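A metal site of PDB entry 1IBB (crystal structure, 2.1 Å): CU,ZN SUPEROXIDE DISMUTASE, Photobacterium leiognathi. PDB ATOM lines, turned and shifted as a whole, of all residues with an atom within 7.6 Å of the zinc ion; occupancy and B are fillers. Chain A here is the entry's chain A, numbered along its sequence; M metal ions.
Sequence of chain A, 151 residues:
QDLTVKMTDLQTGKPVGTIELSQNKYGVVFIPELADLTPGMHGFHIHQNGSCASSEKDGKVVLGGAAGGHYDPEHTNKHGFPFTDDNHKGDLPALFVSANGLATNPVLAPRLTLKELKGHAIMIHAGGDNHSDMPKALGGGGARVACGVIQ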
ATOM      1  N   PHE A  44      20.578  22.554  17.659  1.00  0.00           N
ATOM      2  CA  PHE A  44      20.714  22.397  19.095  1.00  0.00           C
ATOM      3  C   PHE A  44      21.918  23.189  19.553  1.00  0.00           C
ATOM      4  O   PHE A  44      23.053  22.854  19.224  1.00  0.00           O
ATOM      5  CB  PHE A  44      20.901  20.899  19.337  1.00  0.00           C
ATOM      6  CG  PHE A  44      20.786  20.477  20.769  1.00  0.00           C
ATOM      7  CD1 PHE A  44      19.857  21.071  21.609  1.00  0.00           C
ATOM      8  CD2 PHE A  44      21.561  19.435  21.247  1.00  0.00           C
ATOM      9  CE1 PHE A  44      19.698  20.624  22.913  1.00  0.00           C
ATOM     10  CE2 PHE A  44      21.418  18.985  22.545  1.00  0.00           C
ATOM     11  CZ  PHE A  44      20.481  19.577  23.380  1.00  0.00           C
ATOM     12  N   HIS A  45      21.683  24.256  20.309  1.00  0.00           N
ATOM     13  CA  HIS A  45      22.789  25.083  20.791  1.00  0.00           C
ATOM     14  C   HIS A  45      22.608  25.653  22.172  1.00  0.00           C
ATOM     15  O   HIS A  45      21.486  25.762  22.679  1.00  0.00           O
ATOM     16  CB  HIS A  45      23.056  26.290  19.874  1.00  0.00           C
ATOM     17  CG  HIS A  45      22.586  26.119  18.463  1.00  0.00           C
ATOM     18  ND1 HIS A  45      21.391  26.635  18.015  1.00  0.00           N
ATOM     19  CD2 HIS A  45      23.179  25.551  17.383  1.00  0.00           C
ATOM     20  CE1 HIS A  45      21.265  26.394  16.729  1.00  0.00           C
ATOM     21  NE2 HIS A  45      22.334  25.740  16.318  1.00  0.00           N
ATOM     22  N   ILE A  46      23.726  26.040  22.770  1.00  0.00           N
ATOM     23  CA  ILE A  46      23.739  26.675  24.064  1.00  0.00           C
ATOM     24  C   ILE A  46      23.738  28.163  23.752  1.00  0.00           C
ATOM     25  O   ILE A  46      24.539  28.636  22.933  1.00  0.00           O
ATOM     26  CB  ILE A  46      25.008  26.377  24.848  1.00  0.00           C
ATOM     27  CG1 ILE A  46      25.118  24.875  25.151  1.00  0.00           C
ATOM     28  CG2 ILE A  46      25.014  27.188  26.144  1.00  0.00           C
ATOM     29  CD1 ILE A  46      24.006  24.362  26.056  1.00  0.00           C
ATOM     30  N   HIS A  47      22.819  28.906  24.371  1.00  0.00           N
ATOM     31  CA  HIS A  47      22.720  30.349  24.152  1.00  0.00           C
ATOM     32  C   HIS A  47      23.337  31.157  25.302  1.00  0.00           C
ATOM     33  O   HIS A  47      23.517  30.637  26.391  1.00  0.00           O
ATOM     34  CB  HIS A  47      21.271  30.741  23.927  1.00  0.00           C
ATOM     35  CG  HIS A  47      20.805  30.512  22.525  1.00  0.00           C
ATOM     36  ND1 HIS A  47      20.405  31.543  21.698  1.00  0.00           N
ATOM     37  CD2 HIS A  47      20.684  29.379  21.796  1.00  0.00           C
ATOM     38  CE1 HIS A  47      20.070  31.055  20.521  1.00  0.00           C
ATOM     39  NE2 HIS A  47      20.233  29.735  20.555  1.00  0.00           N
ATOM     40  N   GLY A  69      22.048  35.413  21.705  1.00  0.00           N
ATOM     41  CA  GLY A  69      22.647  34.617  20.643  1.00  0.00           C
ATOM     42  C   GLY A  69      23.311  33.353  21.163  1.00  0.00           C
ATOM     43  O   GLY A  69      23.034  32.927  22.295  1.00  0.00           O
ATOM     44  N   HIS A  70      24.172  32.749  20.349  1.00  0.00           N
ATOM     45  CA  HIS A  70      24.875  31.523  20.738  1.00  0.00           C
ATOM     46  C   HIS A  70      26.032  31.796  21.693  1.00  0.00           C
ATOM     47  O   HIS A  70      26.752  32.776  21.531  1.00  0.00           O
ATOM     48  CB  HIS A  70      25.404  30.799  19.502  1.00  0.00           C
ATOM     49  CG  HIS A  70      24.342  30.176  18.651  1.00  0.00           C
ATOM     50  ND1 HIS A  70      24.624  29.523  17.476  1.00  0.00           N
ATOM     51  CD2 HIS A  70      23.000  30.124  18.800  1.00  0.00           C
ATOM     52  CE1 HIS A  70      23.496  29.090  16.933  1.00  0.00           C
ATOM     53  NE2 HIS A  70      22.495  29.440  17.725  1.00  0.00           N
ATOM     54  N   TYR A  71      26.203  30.922  22.669  1.00  0.00           N
ATOM     55  CA  TYR A  71      27.288  31.043  23.635  1.00  0.00           C
ATOM     56  C   TYR A  71      28.576  31.166  22.800  1.00  0.00           C
ATOM     57  O   TYR A  71      28.884  30.296  21.972  1.00  0.00           O
ATOM     58  CB  TYR A  71      27.316  29.792  24.525  1.00  0.00           C
ATOM     59  CG  TYR A  71      28.412  29.744  25.566  1.00  0.00           C
ATOM     60  CD1 TYR A  71      28.583  30.778  26.494  1.00  0.00           C
ATOM     61  CD2 TYR A  71      29.267  28.650  25.643  1.00  0.00           C
ATOM     62  CE1 TYR A  71      29.589  30.710  27.474  1.00  0.00           C
ATOM     63  CE2 TYR A  71      30.271  28.575  26.606  1.00  0.00           C
ATOM     64  CZ  TYR A  71      30.418  29.596  27.517  1.00  0.00           C
ATOM     65  OH  TYR A  71      31.423  29.493  28.467  1.00  0.00           O
ATOM     66  N   ASP A  72      29.301  32.260  23.012  1.00  0.00           N
ATOM     67  CA  ASP A  72      30.519  32.553  22.258  1.00  0.00           C
ATOM     68  C   ASP A  72      31.550  33.326  23.100  1.00  0.00           C
ATOM     69  O   ASP A  72      31.889  34.461  22.792  1.00  0.00           O
ATOM     70  CB  ASP A  72      30.122  33.354  21.014  1.00  0.00           C
ATOM     71  CG  ASP A  72      31.283  33.601  20.055  1.00  0.00           C
ATOM     72  OD1 ASP A  72      32.284  32.851  20.094  1.00  0.00           O
ATOM     73  OD2 ASP A  72      31.183  34.551  19.245  1.00  0.00           O
ATOM     74  N   THR A  76      33.976  34.624  18.640  1.00  0.00           N
ATOM     75  CA  THR A  76      34.312  34.237  17.276  1.00  0.00           C
ATOM     76  C   THR A  76      33.389  34.867  16.246  1.00  0.00           C
ATOM     77  O   THR A  76      33.776  35.079  15.101  1.00  0.00           O
ATOM     78  CB  THR A  76      34.245  32.713  17.094  1.00  0.00           C
ATOM     79  OG1 THR A  76      32.920  32.265  17.398  1.00  0.00           O
ATOM     80  CG2 THR A  76      35.238  32.027  18.005  1.00  0.00           C
ATOM     81  N   LYS A  78      31.136  33.583  14.648  1.00  0.00           N
ATOM     82  CA  LYS A  78      30.863  32.663  13.553  1.00  0.00           C
ATOM     83  C   LYS A  78      30.190  31.413  14.103  1.00  0.00           C
ATOM     84  O   LYS A  78      30.399  31.029  15.250  1.00  0.00           O
ATOM     85  CB  LYS A  78      32.160  32.264  12.841  1.00  0.00           C
ATOM     86  CG  LYS A  78      32.991  33.430  12.364  1.00  0.00           C
ATOM     87  CD  LYS A  78      34.284  32.936  11.758  1.00  0.00           C
ATOM     88  CE  LYS A  78      35.238  34.086  11.508  1.00  0.00           C
ATOM     89  NZ  LYS A  78      36.549  33.579  11.047  1.00  0.00           N
ATOM     90  N   HIS A  79      29.378  30.775  13.256  1.00  0.00           N
ATOM     91  CA  HIS A  79      28.680  29.564  13.646  1.00  0.00           C
ATOM     92  C   HIS A  79      29.368  28.422  12.916  1.00  0.00           C
ATOM     93  O   HIS A  79      29.705  28.548  11.742  1.00  0.00           O
ATOM     94  CB  HIS A  79      27.207  29.649  13.255  1.00  0.00           C
ATOM     95  CG  HIS A  79      26.439  28.380  13.489  1.00  0.00           C
ATOM     96  ND1 HIS A  79      26.004  27.991  14.739  1.00  0.00           N
ATOM     97  CD2 HIS A  79      26.018  27.425  12.625  1.00  0.00           C
ATOM     98  CE1 HIS A  79      25.359  26.843  14.631  1.00  0.00           C
ATOM     99  NE2 HIS A  79      25.358  26.483  13.362  1.00  0.00           N
ATOM    100  N   GLY A  80      29.597  27.311  13.615  1.00  0.00           N
ATOM    101  CA  GLY A  80      30.262  26.187  12.968  1.00  0.00           C
ATOM    102  C   GLY A  80      29.980  24.822  13.568  1.00  0.00           C
ATOM    103  O   GLY A  80      28.909  24.564  14.115  1.00  0.00           O
ATOM    104  N   PHE A  81      30.964  23.940  13.460  1.00  0.00           N
ATOM    105  CA  PHE A  81      30.846  22.576  13.964  1.00  0.00           C
ATOM    106  C   PHE A  81      31.240  22.504  15.447  1.00  0.00           C
ATOM    107  O   PHE A  81      31.830  23.443  15.990  1.00  0.00           O
ATOM    108  CB  PHE A  81      31.742  21.642  13.141  1.00  0.00           C
ATOM    109  CG  PHE A  81      31.354  21.540  11.680  1.00  0.00           C
ATOM    110  CD1 PHE A  81      30.391  20.630  11.254  1.00  0.00           C
ATOM    111  CD2 PHE A  81      31.960  22.372  10.731  1.00  0.00           C
ATOM    112  CE1 PHE A  81      30.020  20.536   9.913  1.00  0.00           C
ATOM    113  CE2 PHE A  81      31.601  22.284   9.386  1.00  0.00           C
ATOM    114  CZ  PHE A  81      30.631  21.365   8.977  1.00  0.00           C
ATOM    115  N   ASN A  87      34.579  29.181  16.107  1.00  0.00           N
ATOM    116  CA  ASN A  87      33.142  29.461  16.048  1.00  0.00           C
ATOM    117  C   ASN A  87      32.504  29.267  17.430  1.00  0.00           C
ATOM    118  O   ASN A  87      33.142  28.753  18.359  1.00  0.00           O
ATOM    119  CB  ASN A  87      32.472  28.548  15.013  1.00  0.00           C
ATOM    120  CG  ASN A  87      32.702  27.085  15.292  1.00  0.00           C
ATOM    121  OD1 ASN A  87      33.632  26.482  14.762  1.00  0.00           O
ATOM    122  ND2 ASN A  87      31.855  26.490  16.126  1.00  0.00           N
ATOM    123  N   HIS A  88      31.259  29.700  17.568  1.00  0.00           N
ATOM    124  CA  HIS A  88      30.530  29.607  18.830  1.00  0.00           C
ATOM    125  C   HIS A  88      30.804  28.312  19.587  1.00  0.00           C
ATOM    126  O   HIS A  88      30.607  27.227  19.055  1.00  0.00           O
ATOM    127  CB  HIS A  88      29.027  29.684  18.590  1.00  0.00           C
ATOM    128  CG  HIS A  88      28.599  30.842  17.756  1.00  0.00           C
ATOM    129  ND1 HIS A  88      27.639  30.730  16.764  1.00  0.00           N
ATOM    130  CD2 HIS A  88      28.948  32.147  17.792  1.00  0.00           C
ATOM    131  CE1 HIS A  88      27.422  31.916  16.241  1.00  0.00           C
ATOM    132  NE2 HIS A  88      28.194  32.795  16.845  1.00  0.00           N
ATOM    133  N   LYS A  89      31.230  28.436  20.835  1.00  0.00           N
ATOM    134  CA  LYS A  89      31.501  27.261  21.628  1.00  0.00           C
ATOM    135  C   LYS A  89      30.160  26.642  22.018  1.00  0.00           C
ATOM    136  O   LYS A  89      30.108  25.516  22.516  1.00  0.00           O
ATOM    137  CB  LYS A  89      32.308  27.630  22.877  1.00  0.00           C
ATOM    138  CG  LYS A  89      33.335  26.553  23.230  1.00  0.00           C
ATOM    139  CD  LYS A  89      33.672  26.496  24.708  1.00  0.00           C
ATOM    140  CE  LYS A  89      34.724  27.512  25.082  1.00  0.00           C
ATOM    141  NZ  LYS A  89      35.132  27.361  26.518  1.00  0.00           N
ATOM    142  N   GLY A  90      29.069  27.374  21.786  1.00  0.00           N
ATOM    143  CA  GLY A  90      27.751  26.861  22.120  1.00  0.00           C
ATOM    144  C   GLY A  90      27.172  25.977  21.031  1.00  0.00           C
ATOM    145  O   GLY A  90      26.066  25.460  21.178  1.00  0.00           O
ATOM    146  N   ASP A  91      27.919  25.799  19.952  1.00  0.00           N
ATOM    147  CA  ASP A  91      27.473  24.973  18.830  1.00  0.00           C
ATOM    148  C   ASP A  91      27.596  23.484  19.170  1.00  0.00           C
ATOM    149  O   ASP A  91      28.711  22.968  19.354  1.00  0.00           O
ATOM    150  CB  ASP A  91      28.283  25.316  17.575  1.00  0.00           C
ATOM    151  CG  ASP A  91      28.075  26.745  17.132  1.00  0.00           C
ATOM    152  OD1 ASP A  91      26.995  27.298  17.439  1.00  0.00           O
ATOM    153  OD2 ASP A  91      28.955  27.332  16.477  1.00  0.00           O
ATOM    154  N   LEU A  92      26.459  22.813  19.249  1.00  0.00           N
ATOM    155  CA  LEU A  92      26.393  21.396  19.579  1.00  0.00           C
ATOM    156  C   LEU A  92      25.987  20.576  18.357  1.00  0.00           C
ATOM    157  O   LEU A  92      25.550  21.131  17.356  1.00  0.00           O
ATOM    158  CB  LEU A  92      25.356  21.172  20.688  1.00  0.00           C
ATOM    159  CG  LEU A  92      25.519  22.006  21.980  1.00  0.00           C
ATOM    160  CD1 LEU A  92      24.344  21.732  22.907  1.00  0.00           C
ATOM    161  CD2 LEU A  92      26.832  21.676  22.646  1.00  0.00           C
ATOM    162  N   ARG A 111      34.309  20.544  23.061  1.00  0.00           N
ATOM    163  CA  ARG A 111      34.863  21.829  23.477  1.00  0.00           C
ATOM    164  C   ARG A 111      34.257  22.411  24.752  1.00  0.00           C
ATOM    165  O   ARG A 111      34.696  23.457  25.224  1.00  0.00           O
ATOM    166  CB  ARG A 111      34.732  22.863  22.372  1.00  0.00           C
ATOM    167  CG  ARG A 111      35.552  22.570  21.121  1.00  0.00           C
ATOM    168  CD  ARG A 111      35.632  23.808  20.247  1.00  0.00           C
ATOM    169  NE  ARG A 111      34.331  24.161  19.682  1.00  0.00           N
ATOM    170  CZ  ARG A 111      33.959  25.399  19.395  1.00  0.00           C
ATOM    171  NH1 ARG A 111      34.782  26.410  19.619  1.00  0.00           N
ATOM    172  NH2 ARG A 111      32.753  25.619  18.888  1.00  0.00           N
ATOM    173  N   ASP A 129      20.590  22.155  11.163  1.00  0.00           N
ATOM    174  CA  ASP A 129      21.846  22.844  11.398  1.00  0.00           C
ATOM    175  C   ASP A 129      22.952  22.280  10.494  1.00  0.00           C
ATOM    176  O   ASP A 129      23.422  21.176  10.724  1.00  0.00           O
ATOM    177  CB  ASP A 129      22.252  22.682  12.864  1.00  0.00           C
ATOM    178  CG  ASP A 129      23.391  23.589  13.280  1.00  0.00           C
ATOM    179  OD1 ASP A 129      24.038  24.192  12.389  1.00  0.00           O
ATOM    180  OD2 ASP A 129      23.653  23.701  14.499  1.00  0.00           O
ATOM    181  N   HIS A 131      25.772  23.644  10.308  1.00  0.00           N
ATOM    182  CA  HIS A 131      26.965  24.210  10.947  1.00  0.00           C
ATOM    183  C   HIS A 131      27.725  25.193  10.070  1.00  0.00           C
ATOM    184  O   HIS A 131      28.929  25.058   9.873  1.00  0.00           O
ATOM    185  CB  HIS A 131      27.899  23.079  11.388  1.00  0.00           C
ATOM    186  CG  HIS A 131      27.239  22.066  12.258  1.00  0.00           C
ATOM    187  ND1 HIS A 131      26.742  20.872  11.769  1.00  0.00           N
ATOM    188  CD2 HIS A 131      26.931  22.078  13.575  1.00  0.00           C
ATOM    189  CE1 HIS A 131      26.163  20.208  12.743  1.00  0.00           C
ATOM    190  NE2 HIS A 131      26.258  20.914  13.856  1.00  0.00           N
ATOM    191  N   ASP A 133      27.124  29.577   8.402  1.00  0.00           N
ATOM    192  CA  ASP A 133      26.263  30.741   8.250  1.00  0.00           C
ATOM    193  C   ASP A 133      25.806  30.854   6.809  1.00  0.00           C
ATOM    194  O   ASP A 133      25.287  31.887   6.389  1.00  0.00           O
ATOM    195  CB  ASP A 133      27.006  32.009   8.679  1.00  0.00           C
ATOM    196  CG  ASP A 133      27.201  32.105  10.186  1.00  0.00           C
ATOM    197  OD1 ASP A 133      26.190  32.083  10.915  1.00  0.00           O
ATOM    198  OD2 ASP A 133      28.358  32.194  10.625  1.00  0.00           O
ATOM    199  N   LEU A 138      23.453  31.066  11.182  1.00  0.00           N
ATOM    200  CA  LEU A 138      23.249  30.184  12.316  1.00  0.00           C
ATOM    201  C   LEU A 138      22.830  28.779  11.898  1.00  0.00           C
ATOM    202  O   LEU A 138      22.021  28.134  12.565  1.00  0.00           O
ATOM    203  CB  LEU A 138      22.199  30.789  13.254  1.00  0.00           C
ATOM    204  CG  LEU A 138      22.457  32.242  13.663  1.00  0.00           C
ATOM    205  CD1 LEU A 138      21.431  32.638  14.708  1.00  0.00           C
ATOM    206  CD2 LEU A 138      23.869  32.406  14.203  1.00  0.00           C
ATOM    207  N   GLY A 139      23.379  28.321  10.782  1.00  0.00           N
ATOM    208  CA  GLY A 139      23.057  26.981  10.307  1.00  0.00           C
ATOM    209  C   GLY A 139      21.640  26.714   9.832  1.00  0.00           C
ATOM    210  O   GLY A 139      21.326  25.580   9.477  1.00  0.00           O
HETATM  211 ZN    ZN M   1      26.456  28.933  16.693  1.00  0.00          ZN
HETATM  212 CU    CU M   2      20.353  28.269  18.870  1.00  0.00          CU
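The backbone NH (N) of Gly 80 lies within hydrogen-bond range of the side-chain carboxylate (OD2) of Asp 91 (2.9 Å).
The side-chain carboxylate of Asp 91 is in hydrogen-bond range of the side-chain amide nitrogen of Asn 87, 3.0 Å away.
The guanidinium group of Arg 111 sits at hydrogen-bond distance from the backbone carbonyl oxygen of His 88 (2.7 Å).
The backbone NH of His 88 is in hydrogen-bond range of the backbone carbonyl oxygen of Lys 78, at 2.8 Å.
A ring nitrogen (NE2) of His 70 lies close to a ring nitrogen (ND1) of His 45, 3.0 Å away.
The side-chain hydroxyl of Thr 76 is in hydrogen-bond range of the backbone NH of His 88, at 3.1 Å.
The backbone NH (N) of His 79 is in hydrogen-bond range of the side-chain carboxylate (OD2) of Asp 133.
The side-chain carboxylate of Asp 129 sits at hydrogen-bond distance from a ring nitrogen (NE2) of His 79 (2.8 Å).
Of the 25 residues printed, 4 come within 4 Å of the zinc ion.
The zinc ion is bound by OD1 of Asp 91, ND1 of His 70, ND1 of His 88 and ND1 of His 79.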
